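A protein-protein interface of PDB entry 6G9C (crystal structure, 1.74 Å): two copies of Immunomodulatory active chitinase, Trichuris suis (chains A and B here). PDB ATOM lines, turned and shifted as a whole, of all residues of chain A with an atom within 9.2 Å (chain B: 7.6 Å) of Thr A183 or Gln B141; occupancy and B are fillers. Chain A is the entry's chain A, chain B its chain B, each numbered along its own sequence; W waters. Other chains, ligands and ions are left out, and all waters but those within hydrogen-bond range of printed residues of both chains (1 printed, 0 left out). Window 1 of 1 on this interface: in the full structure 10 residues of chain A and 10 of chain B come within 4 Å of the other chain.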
ATOM      1  N   GLN A 141      19.905 -12.161  -0.209  1.00  0.00           N
ATOM      2  CA  GLN A 141      20.182 -13.101  -1.291  1.00  0.00           C
ATOM      3  C   GLN A 141      19.807 -14.526  -0.903  1.00  0.00           C
ATOM      4  O   GLN A 141      19.318 -15.288  -1.745  1.00  0.00           O
ATOM      5  CB  GLN A 141      21.655 -13.029  -1.719  1.00  0.00           C
ATOM      6  CG  GLN A 141      22.028 -11.727  -2.433  1.00  0.00           C
ATOM      7  CD  GLN A 141      22.889 -11.944  -3.686  1.00  0.00           C
ATOM      8  OE1 GLN A 141      23.850 -12.711  -3.670  1.00  0.00           O
ATOM      9  NE2 GLN A 141      22.548 -11.248  -4.769  1.00  0.00           N
ATOM     10  N   LYS A 144      16.039 -14.723  -1.520  1.00  0.00           N
ATOM     11  CA  LYS A 144      15.570 -14.439  -2.877  1.00  0.00           C
ATOM     12  C   LYS A 144      14.837 -13.108  -2.976  1.00  0.00           C
ATOM     13  O   LYS A 144      13.980 -12.938  -3.843  1.00  0.00           O
ATOM     14  CB  LYS A 144      14.667 -15.568  -3.408  1.00  0.00           C
ATOM     15  CG  LYS A 144      15.252 -16.964  -3.266  1.00  0.00           C
ATOM     16  CD  LYS A 144      16.522 -17.113  -4.066  1.00  0.00           C
ATOM     17  CE  LYS A 144      16.592 -18.492  -4.713  1.00  0.00           C
ATOM     18  NZ  LYS A 144      16.463 -19.589  -3.717  1.00  0.00           N
ATOM     19  N   PHE A 145      15.150 -12.154  -2.101  1.00  0.00           N
ATOM     20  CA  PHE A 145      14.535 -10.840  -2.200  1.00  0.00           C
ATOM     21  C   PHE A 145      15.116 -10.051  -3.373  1.00  0.00           C
ATOM     22  O   PHE A 145      16.256 -10.265  -3.808  1.00  0.00           O
ATOM     23  CB  PHE A 145      14.707 -10.055  -0.891  1.00  0.00           C
ATOM     24  CG  PHE A 145      13.764 -10.502   0.194  1.00  0.00           C
ATOM     25  CD1 PHE A 145      12.457 -10.035   0.225  1.00  0.00           C
ATOM     26  CD2 PHE A 145      14.170 -11.415   1.151  1.00  0.00           C
ATOM     27  CE1 PHE A 145      11.567 -10.464   1.202  1.00  0.00           C
ATOM     28  CE2 PHE A 145      13.288 -11.842   2.144  1.00  0.00           C
ATOM     29  CZ  PHE A 145      11.985 -11.371   2.162  1.00  0.00           C
ATOM     30  N   ASP A 146      14.299  -9.142  -3.897  1.00  0.00           N
ATOM     31  CA  ASP A 146      14.677  -8.243  -4.978  1.00  0.00           C
ATOM     32  C   ASP A 146      15.216  -6.909  -4.480  1.00  0.00           C
ATOM     33  O   ASP A 146      15.685  -6.107  -5.294  1.00  0.00           O
ATOM     34  CB  ASP A 146      13.462  -7.981  -5.871  1.00  0.00           C
ATOM     35  CG  ASP A 146      12.983  -9.237  -6.559  1.00  0.00           C
ATOM     36  OD1 ASP A 146      13.785  -9.840  -7.307  1.00  0.00           O
ATOM     37  OD2 ASP A 146      11.827  -9.653  -6.309  1.00  0.00           O
ATOM     38  N   LYS A 173      27.336  -1.266  -1.466  1.00  0.00           N
ATOM     39  CA  LYS A 173      27.430  -2.715  -1.315  1.00  0.00           C
ATOM     40  C   LYS A 173      26.556  -3.425  -2.334  1.00  0.00           C
ATOM     41  O   LYS A 173      26.974  -4.431  -2.927  1.00  0.00           O
ATOM     42  CB  LYS A 173      27.020  -3.142   0.091  1.00  0.00           C
ATOM     43  CG  LYS A 173      27.227  -4.627   0.363  1.00  0.00           C
ATOM     44  CD  LYS A 173      28.716  -4.957   0.362  1.00  0.00           C
ATOM     45  CE  LYS A 173      29.022  -6.207   1.173  1.00  0.00           C
ATOM     46  NZ  LYS A 173      30.225  -6.946   0.689  1.00  0.00           N
ATOM     47  N   PHE A 174      25.334  -2.919  -2.539  1.00  0.00           N
ATOM     48  CA  PHE A 174      24.421  -3.543  -3.501  1.00  0.00           C
ATOM     49  C   PHE A 174      25.043  -3.551  -4.893  1.00  0.00           C
ATOM     50  O   PHE A 174      24.965  -4.552  -5.618  1.00  0.00           O
ATOM     51  CB  PHE A 174      23.066  -2.814  -3.514  1.00  0.00           C
ATOM     52  CG  PHE A 174      22.155  -3.144  -2.339  1.00  0.00           C
ATOM     53  CD1 PHE A 174      22.602  -3.916  -1.271  1.00  0.00           C
ATOM     54  CD2 PHE A 174      20.837  -2.687  -2.315  1.00  0.00           C
ATOM     55  CE1 PHE A 174      21.755  -4.217  -0.203  1.00  0.00           C
ATOM     56  CE2 PHE A 174      19.992  -2.980  -1.246  1.00  0.00           C
ATOM     57  CZ  PHE A 174      20.458  -3.740  -0.188  1.00  0.00           C
ATOM     58  N   GLU A 175      25.697  -2.451  -5.273  1.00  0.00           N
ATOM     59  CA  GLU A 175      26.361  -2.393  -6.573  1.00  0.00           C
ATOM     60  C   GLU A 175      27.520  -3.380  -6.652  1.00  0.00           C
ATOM     61  O   GLU A 175      27.724  -4.030  -7.686  1.00  0.00           O
ATOM     62  CB  GLU A 175      26.843  -0.963  -6.840  1.00  0.00           C
ATOM     63  CG  GLU A 175      25.684  -0.007  -7.120  1.00  0.00           C
ATOM     64  CD  GLU A 175      26.088   1.448  -7.097  1.00  0.00           C
ATOM     65  OE1 GLU A 175      27.151   1.771  -6.525  1.00  0.00           O
ATOM     66  OE2 GLU A 175      25.330   2.273  -7.647  1.00  0.00           O
ATOM     67  N   GLU A 176      28.297  -3.500  -5.573  1.00  0.00           N
ATOM     68  CA  GLU A 176      29.417  -4.435  -5.567  1.00  0.00           C
ATOM     69  C   GLU A 176      28.923  -5.880  -5.601  1.00  0.00           C
ATOM     70  O   GLU A 176      29.502  -6.735  -6.287  1.00  0.00           O
ATOM     71  CB  GLU A 176      30.287  -4.180  -4.333  1.00  0.00           C
ATOM     72  CG  GLU A 176      31.393  -5.199  -4.090  1.00  0.00           C
ATOM     73  CD  GLU A 176      31.548  -5.551  -2.611  1.00  0.00           C
ATOM     74  OE1 GLU A 176      31.171  -6.681  -2.218  1.00  0.00           O
ATOM     75  OE2 GLU A 176      32.033  -4.693  -1.840  1.00  0.00           O
ATOM     76  N   VAL A 177      27.860  -6.168  -4.859  1.00  0.00           N
ATOM     77  CA  VAL A 177      27.291  -7.513  -4.866  1.00  0.00           C
ATOM     78  C   VAL A 177      26.798  -7.874  -6.261  1.00  0.00           C
ATOM     79  O   VAL A 177      26.999  -9.002  -6.734  1.00  0.00           O
ATOM     80  CB  VAL A 177      26.180  -7.613  -3.806  1.00  0.00           C
ATOM     81  CG1 VAL A 177      25.300  -8.835  -4.031  1.00  0.00           C
ATOM     82  CG2 VAL A 177      26.811  -7.647  -2.421  1.00  0.00           C
ATOM     83  N   ALA A 178      26.189  -6.911  -6.957  1.00  0.00           N
ATOM     84  CA  ALA A 178      25.727  -7.164  -8.319  1.00  0.00           C
ATOM     85  C   ALA A 178      26.870  -7.600  -9.224  1.00  0.00           C
ATOM     86  O   ALA A 178      26.721  -8.558  -9.993  1.00  0.00           O
ATOM     87  CB  ALA A 178      25.022  -5.925  -8.878  1.00  0.00           C
ATOM     88  N   LYS A 179      28.041  -6.932  -9.131  1.00  0.00           N
ATOM     89  CA  LYS A 179      29.186  -7.335  -9.932  1.00  0.00           C
ATOM     90  C   LYS A 179      29.735  -8.680  -9.474  1.00  0.00           C
ATOM     91  O   LYS A 179      30.130  -9.507 -10.301  1.00  0.00           O
ATOM     92  CB  LYS A 179      30.291  -6.269  -9.854  1.00  0.00           C
ATOM     93  CG  LYS A 179      29.821  -4.865 -10.205  1.00  0.00           C
ATOM     94  CD  LYS A 179      30.936  -3.831 -10.011  1.00  0.00           C
ATOM     95  CE  LYS A 179      30.523  -2.448 -10.524  1.00  0.00           C
ATOM     96  NZ  LYS A 179      30.112  -1.489  -9.461  1.00  0.00           N
ATOM     97  N   CYS A 180      29.799  -8.897  -8.158  1.00  0.00           N
ATOM     98  CA  CYS A 180      30.390 -10.122  -7.622  1.00  0.00           C
ATOM     99  C   CYS A 180      29.610 -11.362  -8.055  1.00  0.00           C
ATOM    100  O   CYS A 180      30.202 -12.412  -8.339  1.00  0.00           O
ATOM    101  CB  CYS A 180      30.445 -10.041  -6.091  1.00  0.00           C
ATOM    102  SG  CYS A 180      31.527 -11.265  -5.282  1.00  0.00           S
ATOM    103  N   THR A 181      28.282 -11.262  -8.104  1.00  0.00           N
ATOM    104  CA  THR A 181      27.424 -12.408  -8.389  1.00  0.00           C
ATOM    105  C   THR A 181      26.837 -12.394  -9.795  1.00  0.00           C
ATOM    106  O   THR A 181      26.029 -13.271 -10.115  1.00  0.00           O
ATOM    107  CB  THR A 181      26.286 -12.485  -7.367  1.00  0.00           C
ATOM    108  OG1 THR A 181      25.513 -11.282  -7.413  1.00  0.00           O
ATOM    109  CG2 THR A 181      26.834 -12.679  -5.970  1.00  0.00           C
ATOM    110  N   SER A 182      27.220 -11.430 -10.630  1.00  0.00           N
ATOM    111  CA  SER A 182      26.699 -11.281 -11.992  1.00  0.00           C
ATOM    112  C   SER A 182      25.172 -11.222 -12.012  1.00  0.00           C
ATOM    113  O   SER A 182      24.506 -11.898 -12.802  1.00  0.00           O
ATOM    114  CB  SER A 182      27.216 -12.398 -12.895  1.00  0.00           C
ATOM    115  OG  SER A 182      28.628 -12.431 -12.895  1.00  0.00           O
ATOM    116  N   THR A 183      24.609 -10.392 -11.136  1.00  0.00           N
ATOM    117  CA  THR A 183      23.165 -10.216 -11.058  1.00  0.00           C
ATOM    118  C   THR A 183      22.816  -8.736 -11.169  1.00  0.00           C
ATOM    119  O   THR A 183      23.677  -7.865 -11.026  1.00  0.00           O
ATOM    120  CB  THR A 183      22.587 -10.791  -9.750  1.00  0.00           C
ATOM    121  OG1 THR A 183      23.068 -10.033  -8.635  1.00  0.00           O
ATOM    122  CG2 THR A 183      22.981 -12.254  -9.568  1.00  0.00           C
ATOM    123  N   SER A 184      21.541  -8.462 -11.447  1.00  0.00           N
ATOM    124  CA  SER A 184      21.033  -7.097 -11.368  1.00  0.00           C
ATOM    125  C   SER A 184      21.031  -6.648  -9.918  1.00  0.00           C
ATOM    126  O   SER A 184      20.698  -7.420  -9.017  1.00  0.00           O
ATOM    127  CB  SER A 184      19.608  -7.006 -11.926  1.00  0.00           C
ATOM    128  OG  SER A 184      19.553  -7.528 -13.237  1.00  0.00           O
ATOM    129  N   ARG A 185      21.389  -5.393  -9.683  1.00  0.00           N
ATOM    130  CA  ARG A 185      21.550  -4.985  -8.297  1.00  0.00           C
ATOM    131  C   ARG A 185      20.204  -4.929  -7.571  1.00  0.00           C
ATOM    132  O   ARG A 185      19.144  -4.669  -8.160  1.00  0.00           O
ATOM    133  CB  ARG A 185      22.275  -3.648  -8.205  1.00  0.00           C
ATOM    134  CG  ARG A 185      21.422  -2.450  -8.426  1.00  0.00           C
ATOM    135  CD  ARG A 185      21.891  -1.322  -7.533  1.00  0.00           C
ATOM    136  NE  ARG A 185      21.314  -0.060  -7.969  1.00  0.00           N
ATOM    137  CZ  ARG A 185      20.138   0.412  -7.563  1.00  0.00           C
ATOM    138  NH1 ARG A 185      19.397  -0.259  -6.686  1.00  0.00           N
ATOM    139  NH2 ARG A 185      19.703   1.573  -8.032  1.00  0.00           N
ATOM    140  N   LEU A 186      20.268  -5.206  -6.276  1.00  0.00           N
ATOM    141  CA  LEU A 186      19.112  -5.108  -5.406  1.00  0.00           C
ATOM    142  C   LEU A 186      18.554  -3.689  -5.406  1.00  0.00           C
ATOM    143  O   LEU A 186      19.303  -2.708  -5.448  1.00  0.00           O
ATOM    144  CB  LEU A 186      19.514  -5.521  -3.992  1.00  0.00           C
ATOM    145  CG  LEU A 186      19.883  -6.993  -3.847  1.00  0.00           C
ATOM    146  CD1 LEU A 186      20.831  -7.194  -2.676  1.00  0.00           C
ATOM    147  CD2 LEU A 186      18.595  -7.785  -3.650  1.00  0.00           C
ATOM    148  N   SER B 135      30.095 -15.322 -19.383  1.00  0.00           N
ATOM    149  CA  SER B 135      28.814 -15.227 -20.067  1.00  0.00           C
ATOM    150  C   SER B 135      27.815 -16.223 -19.494  1.00  0.00           C
ATOM    151  O   SER B 135      26.632 -15.901 -19.320  1.00  0.00           O
ATOM    152  CB  SER B 135      29.012 -15.464 -21.562  1.00  0.00           C
ATOM    153  OG  SER B 135      27.780 -15.453 -22.251  1.00  0.00           O
ATOM    154  N   LEU B 136      28.282 -17.436 -19.192  1.00  0.00           N
ATOM    155  CA  LEU B 136      27.416 -18.473 -18.647  1.00  0.00           C
ATOM    156  C   LEU B 136      26.835 -18.063 -17.299  1.00  0.00           C
ATOM    157  O   LEU B 136      25.624 -18.190 -17.066  1.00  0.00           O
ATOM    158  CB  LEU B 136      28.197 -19.777 -18.506  1.00  0.00           C
ATOM    159  CG  LEU B 136      27.462 -20.869 -17.734  1.00  0.00           C
ATOM    160  CD1 LEU B 136      26.238 -21.393 -18.522  1.00  0.00           C
ATOM    161  CD2 LEU B 136      28.418 -21.996 -17.396  1.00  0.00           C
ATOM    162  N   VAL B 137      27.692 -17.581 -16.394  1.00  0.00           N
ATOM    163  CA  VAL B 137      27.245 -17.259 -15.043  1.00  0.00           C
ATOM    164  C   VAL B 137      26.200 -16.154 -15.081  1.00  0.00           C
ATOM    165  O   VAL B 137      25.171 -16.232 -14.394  1.00  0.00           O
ATOM    166  CB  VAL B 137      28.454 -16.891 -14.157  1.00  0.00           C
ATOM    167  CG1 VAL B 137      28.013 -16.046 -12.979  1.00  0.00           C
ATOM    168  CG2 VAL B 137      29.129 -18.166 -13.677  1.00  0.00           C
ATOM    169  N   SER B 138      26.420 -15.128 -15.911  1.00  0.00           N
ATOM    170  CA  SER B 138      25.412 -14.078 -16.043  1.00  0.00           C
ATOM    171  C   SER B 138      24.113 -14.651 -16.579  1.00  0.00           C
ATOM    172  O   SER B 138      23.028 -14.300 -16.105  1.00  0.00           O
ATOM    173  CB  SER B 138      25.895 -12.962 -16.964  1.00  0.00           C
ATOM    174  OG  SER B 138      27.137 -12.437 -16.522  1.00  0.00           O
ATOM    175  N   PHE B 139      24.207 -15.543 -17.563  1.00  0.00           N
ATOM    176  CA  PHE B 139      22.996 -16.124 -18.134  1.00  0.00           C
ATOM    177  C   PHE B 139      22.245 -16.977 -17.115  1.00  0.00           C
ATOM    178  O   PHE B 139      21.009 -16.928 -17.050  1.00  0.00           O
ATOM    179  CB  PHE B 139      23.346 -16.949 -19.368  1.00  0.00           C
ATOM    180  CG  PHE B 139      22.151 -17.311 -20.212  1.00  0.00           C
ATOM    181  CD1 PHE B 139      21.672 -16.433 -21.173  1.00  0.00           C
ATOM    182  CD2 PHE B 139      21.515 -18.529 -20.048  1.00  0.00           C
ATOM    183  CE1 PHE B 139      20.569 -16.772 -21.966  1.00  0.00           C
ATOM    184  CE2 PHE B 139      20.404 -18.872 -20.836  1.00  0.00           C
ATOM    185  CZ  PHE B 139      19.941 -17.989 -21.788  1.00  0.00           C
ATOM    186  N   LEU B 140      22.969 -17.784 -16.333  1.00  0.00           N
ATOM    187  CA  LEU B 140      22.330 -18.592 -15.295  1.00  0.00           C
ATOM    188  C   LEU B 140      21.636 -17.718 -14.257  1.00  0.00           C
ATOM    189  O   LEU B 140      20.498 -18.004 -13.857  1.00  0.00           O
ATOM    190  CB  LEU B 140      23.362 -19.492 -14.612  1.00  0.00           C
ATOM    191  CG  LEU B 140      24.013 -20.570 -15.480  1.00  0.00           C
ATOM    192  CD1 LEU B 140      25.096 -21.278 -14.693  1.00  0.00           C
ATOM    193  CD2 LEU B 140      22.978 -21.587 -15.998  1.00  0.00           C
ATOM    194  N   GLN B 141      22.310 -16.651 -13.809  1.00  0.00           N
ATOM    195  CA  GLN B 141      21.764 -15.798 -12.757  1.00  0.00           C
ATOM    196  C   GLN B 141      20.549 -15.021 -13.246  1.00  0.00           C
ATOM    197  O   GLN B 141      19.509 -14.991 -12.576  1.00  0.00           O
ATOM    198  CB  GLN B 141      22.847 -14.840 -12.238  1.00  0.00           C
ATOM    199  CG  GLN B 141      24.051 -15.543 -11.609  1.00  0.00           C
ATOM    200  CD  GLN B 141      23.761 -16.088 -10.221  1.00  0.00           C
ATOM    201  OE1 GLN B 141      22.966 -17.018 -10.061  1.00  0.00           O
ATOM    202  NE2 GLN B 141      24.403 -15.509  -9.207  1.00  0.00           N
ATOM    203  N   GLN B 142      20.659 -14.390 -14.418  1.00  0.00           N
ATOM    204  CA  GLN B 142      19.555 -13.592 -14.944  1.00  0.00           C
ATOM    205  C   GLN B 142      18.287 -14.422 -15.115  1.00  0.00           C
ATOM    206  O   GLN B 142      17.179 -13.899 -14.961  1.00  0.00           O
ATOM    207  CB  GLN B 142      19.950 -12.965 -16.283  1.00  0.00           C
ATOM    208  CG  GLN B 142      21.087 -11.953 -16.192  1.00  0.00           C
ATOM    209  CD  GLN B 142      21.712 -11.642 -17.545  1.00  0.00           C
ATOM    210  OE1 GLN B 142      21.370 -12.253 -18.562  1.00  0.00           O
ATOM    211  NE2 GLN B 142      22.637 -10.687 -17.560  1.00  0.00           N
ATOM    212  N   ASN B 143      18.425 -15.708 -15.419  1.00  0.00           N
ATOM    213  CA  ASN B 143      17.285 -16.550 -15.748  1.00  0.00           C
ATOM    214  C   ASN B 143      16.923 -17.508 -14.621  1.00  0.00           C
ATOM    215  O   ASN B 143      16.037 -18.356 -14.798  1.00  0.00           O
ATOM    216  CB  ASN B 143      17.572 -17.281 -17.056  1.00  0.00           C
ATOM    217  CG  ASN B 143      17.645 -16.319 -18.231  1.00  0.00           C
ATOM    218  OD1 ASN B 143      16.643 -15.701 -18.599  1.00  0.00           O
ATOM    219  ND2 ASN B 143      18.834 -16.156 -18.803  1.00  0.00           N
ATOM    220  N   LYS B 144      17.590 -17.373 -13.463  1.00  0.00           N
ATOM    221  CA  LYS B 144      17.207 -17.998 -12.191  1.00  0.00           C
ATOM    222  C   LYS B 144      17.434 -19.505 -12.185  1.00  0.00           C
ATOM    223  O   LYS B 144      16.704 -20.243 -11.521  1.00  0.00           O
ATOM    224  CB  LYS B 144      15.751 -17.683 -11.826  1.00  0.00           C
ATOM    225  CG  LYS B 144      15.423 -16.193 -11.827  1.00  0.00           C
ATOM    226  CD  LYS B 144      16.216 -15.475 -10.765  1.00  0.00           C
ATOM    227  CE  LYS B 144      15.952 -13.977 -10.791  1.00  0.00           C
ATOM    228  NZ  LYS B 144      14.491 -13.696 -10.864  1.00  0.00           N
ATOM    229  N   PHE B 145      18.456 -19.971 -12.896  1.00  0.00           N
ATOM    230  CA  PHE B 145      18.793 -21.387 -12.904  1.00  0.00           C
ATOM    231  C   PHE B 145      19.525 -21.779 -11.626  1.00  0.00           C
ATOM    232  O   PHE B 145      20.192 -20.960 -10.981  1.00  0.00           O
ATOM    233  CB  PHE B 145      19.649 -21.731 -14.121  1.00  0.00           C
ATOM    234  CG  PHE B 145      18.859 -21.839 -15.408  1.00  0.00           C
ATOM    235  CD1 PHE B 145      18.140 -22.992 -15.706  1.00  0.00           C
ATOM    236  CD2 PHE B 145      18.832 -20.784 -16.309  1.00  0.00           C
ATOM    237  CE1 PHE B 145      17.407 -23.094 -16.894  1.00  0.00           C
ATOM    238  CE2 PHE B 145      18.105 -20.874 -17.491  1.00  0.00           C
ATOM    239  CZ  PHE B 145      17.393 -22.035 -17.783  1.00  0.00           C
ATOM    240  N   ASP B 146      19.398 -23.053 -11.265  1.00  0.00           N
ATOM    241  CA  ASP B 146      20.034 -23.580 -10.065  1.00  0.00           C
ATOM    242  C   ASP B 146      21.387 -24.224 -10.339  1.00  0.00           C
ATOM    243  O   ASP B 146      22.073 -24.622  -9.395  1.00  0.00           O
ATOM    244  CB  ASP B 146      19.107 -24.596  -9.398  1.00  0.00           C
ATOM    245  CG  ASP B 146      17.798 -23.983  -8.978  1.00  0.00           C
ATOM    246  OD1 ASP B 146      17.827 -23.118  -8.072  1.00  0.00           O
ATOM    247  OD2 ASP B 146      16.745 -24.360  -9.551  1.00  0.00           O
ATOM    248  N   GLY B 147      21.789 -24.336 -11.595  1.00  0.00           N
ATOM    249  CA  GLY B 147      23.035 -25.000 -11.903  1.00  0.00           C
ATOM    250  C   GLY B 147      23.176 -25.184 -13.398  1.00  0.00           C
ATOM    251  O   GLY B 147      22.354 -24.703 -14.192  1.00  0.00           O
ATOM    252  N   VAL B 177      31.192 -17.221  -6.647  1.00  0.00           N
ATOM    253  CA  VAL B 177      29.917 -16.517  -6.639  1.00  0.00           C
ATOM    254  C   VAL B 177      29.202 -16.742  -5.319  1.00  0.00           C
ATOM    255  O   VAL B 177      28.668 -15.803  -4.713  1.00  0.00           O
ATOM    256  CB  VAL B 177      29.061 -16.975  -7.834  1.00  0.00           C
ATOM    257  CG1 VAL B 177      27.572 -16.787  -7.543  1.00  0.00           C
ATOM    258  CG2 VAL B 177      29.478 -16.234  -9.094  1.00  0.00           C
ATOM    259  N   ALA B 178      29.210 -17.987  -4.838  1.00  0.00           N
ATOM    260  CA  ALA B 178      28.537 -18.307  -3.586  1.00  0.00           C
ATOM    261  C   ALA B 178      29.193 -17.611  -2.408  1.00  0.00           C
ATOM    262  O   ALA B 178      28.500 -17.190  -1.474  1.00  0.00           O
ATOM    263  CB  ALA B 178      28.520 -19.819  -3.371  1.00  0.00           C
ATOM    264  N   THR B 181      28.121 -13.826  -0.876  1.00  0.00           N
ATOM    265  CA  THR B 181      26.983 -13.578  -0.003  1.00  0.00           C
ATOM    266  C   THR B 181      26.744 -14.716   0.983  1.00  0.00           C
ATOM    267  O   THR B 181      25.733 -14.695   1.698  1.00  0.00           O
ATOM    268  CB  THR B 181      25.723 -13.374  -0.855  1.00  0.00           C
ATOM    269  OG1 THR B 181      25.713 -14.333  -1.914  1.00  0.00           O
ATOM    270  CG2 THR B 181      25.747 -12.006  -1.487  1.00  0.00           C
ATOM    271  N   THR B 183      25.779 -17.794   0.019  1.00  0.00           N
ATOM    272  CA  THR B 183      24.627 -18.519  -0.496  1.00  0.00           C
ATOM    273  C   THR B 183      25.074 -19.903  -0.953  1.00  0.00           C
ATOM    274  O   THR B 183      26.268 -20.182  -1.079  1.00  0.00           O
ATOM    275  CB  THR B 183      23.964 -17.760  -1.654  1.00  0.00           C
ATOM    276  OG1 THR B 183      24.922 -17.537  -2.701  1.00  0.00           O
ATOM    277  CG2 THR B 183      23.399 -16.418  -1.174  1.00  0.00           C
ATOM    278  N   SER B 184      24.107 -20.780  -1.201  1.00  0.00           N
ATOM    279  CA  SER B 184      24.447 -22.090  -1.738  1.00  0.00           C
ATOM    280  C   SER B 184      24.861 -21.946  -3.198  1.00  0.00           C
ATOM    281  O   SER B 184      24.298 -21.141  -3.942  1.00  0.00           O
ATOM    282  CB  SER B 184      23.274 -23.052  -1.611  1.00  0.00           C
ATOM    283  OG  SER B 184      22.093 -22.436  -2.068  1.00  0.00           O
ATOM    284  N   LEU B 186      25.749 -22.672  -7.203  1.00  0.00           N
ATOM    285  CA  LEU B 186      25.160 -23.314  -8.364  1.00  0.00           C
ATOM    286  C   LEU B 186      25.670 -24.743  -8.480  1.00  0.00           C
ATOM    287  O   LEU B 186      26.827 -25.033  -8.165  1.00  0.00           O
ATOM    288  CB  LEU B 186      25.509 -22.525  -9.625  1.00  0.00           C
ATOM    289  CG  LEU B 186      24.887 -21.133  -9.697  1.00  0.00           C
ATOM    290  CD1 LEU B 186      25.698 -20.236 -10.632  1.00  0.00           C
ATOM    291  CD2 LEU B 186      23.423 -21.237 -10.144  1.00  0.00           C
HETATM  292  O   HOH W   1      23.948 -15.151  -5.776  1.00  0.00           O
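Gln A141 touches Thr B181, and with the chains exchanged Thr A181 touches Gln B141.
Gln A141 touches Thr B183, and with the chains exchanged Thr A183 touches Gln B141.
Thr A181 touches Val B177, but with the chains exchanged Val A177 does not touch Thr B181 (4.1 Å).
10 positions are printed for both chains.
The side-chain amide oxygen (OE1) of Gln A141 sits close to the side-chain hydroxyl (OG1) of Thr B181, at 3.0 Å.
NE2 of Gln B141 sits at hydrogen-bond distance from O of Thr A181 (2.9 Å).
Water W1 lies within hydrogen-bond range of OE1 of Gln A141 (3.2 Å) and NE2 of Gln B141 (3.5 Å).
The backbone carbonyl oxygen (O) of Val A177 sits at hydrogen-bond distance from the side-chain hydroxyl (OG1) of Thr A181.
O of Ala A178 lies within hydrogen-bond range of N of Thr A183 (3.0 Å).
The side-chain hydroxyl of Thr A181 is in hydrogen-bond range of the side-chain hydroxyl of Thr A183.
The backbone carbonyl oxygen of Ala B178 sits at hydrogen-bond distance from the backbone NH of Thr B183, at 3.2 Å.
The side-chain hydroxyl (OG1) of Thr B181 sits close to the side-chain hydroxyl (OG1) of Thr B183.
Printed residues of chain B that touch a printed residue of chain A: Val B137, Ser B138, Gln B141, Val B177, Thr B181 and Thr B183.
Hydrophobic or aromatic side chains of chain B that line the printed part of chain A: Val B137 and Val B177.
Printed residues of chain A that touch a printed residue of chain B: Gln A141, Cys A180, Thr A181, Ser A182 and Thr A183.
Among the printed residues, no Asp or Glu carboxylate lies within 4 Å of a Lys or Arg side-chain nitrogen of the other chain.
Thr A183 touches one residue of chain B.
Of chain A, only Thr A181, Ser A182 and Thr A183 come within 4 Å of Gln B141.
Of the printed residues of chain B, Thr A181 touches Gln B141 (2.9 Å) and Val B177 (3.8 Å).
Of the printed residues of chain B, Cys A180 touches Val B177 (3.96 Å).
Printed residues of chain B within 4 Å of Gln A141: Thr B181 (3.0 Å) and Thr B183 (3.9 Å).
Ser B184 touches none of the printed residues of chain A.
The nearest residue of chain B that does not touch Thr A183 is Gln B142 (5.8 Å).
The nearest printed residue of chain A that does not touch Thr B183 is Thr A181 (6.2 Å).
Among the printed residues, pairs that only touch across the chains: Gln A141 with Thr B183, Cys A180 with Val B177, Thr A181 with Val B177, Ser A182 with Val B137, Ser A182 with Ser B138, Ser A182 with Gln B141 and Thr A183 with Gln B141.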
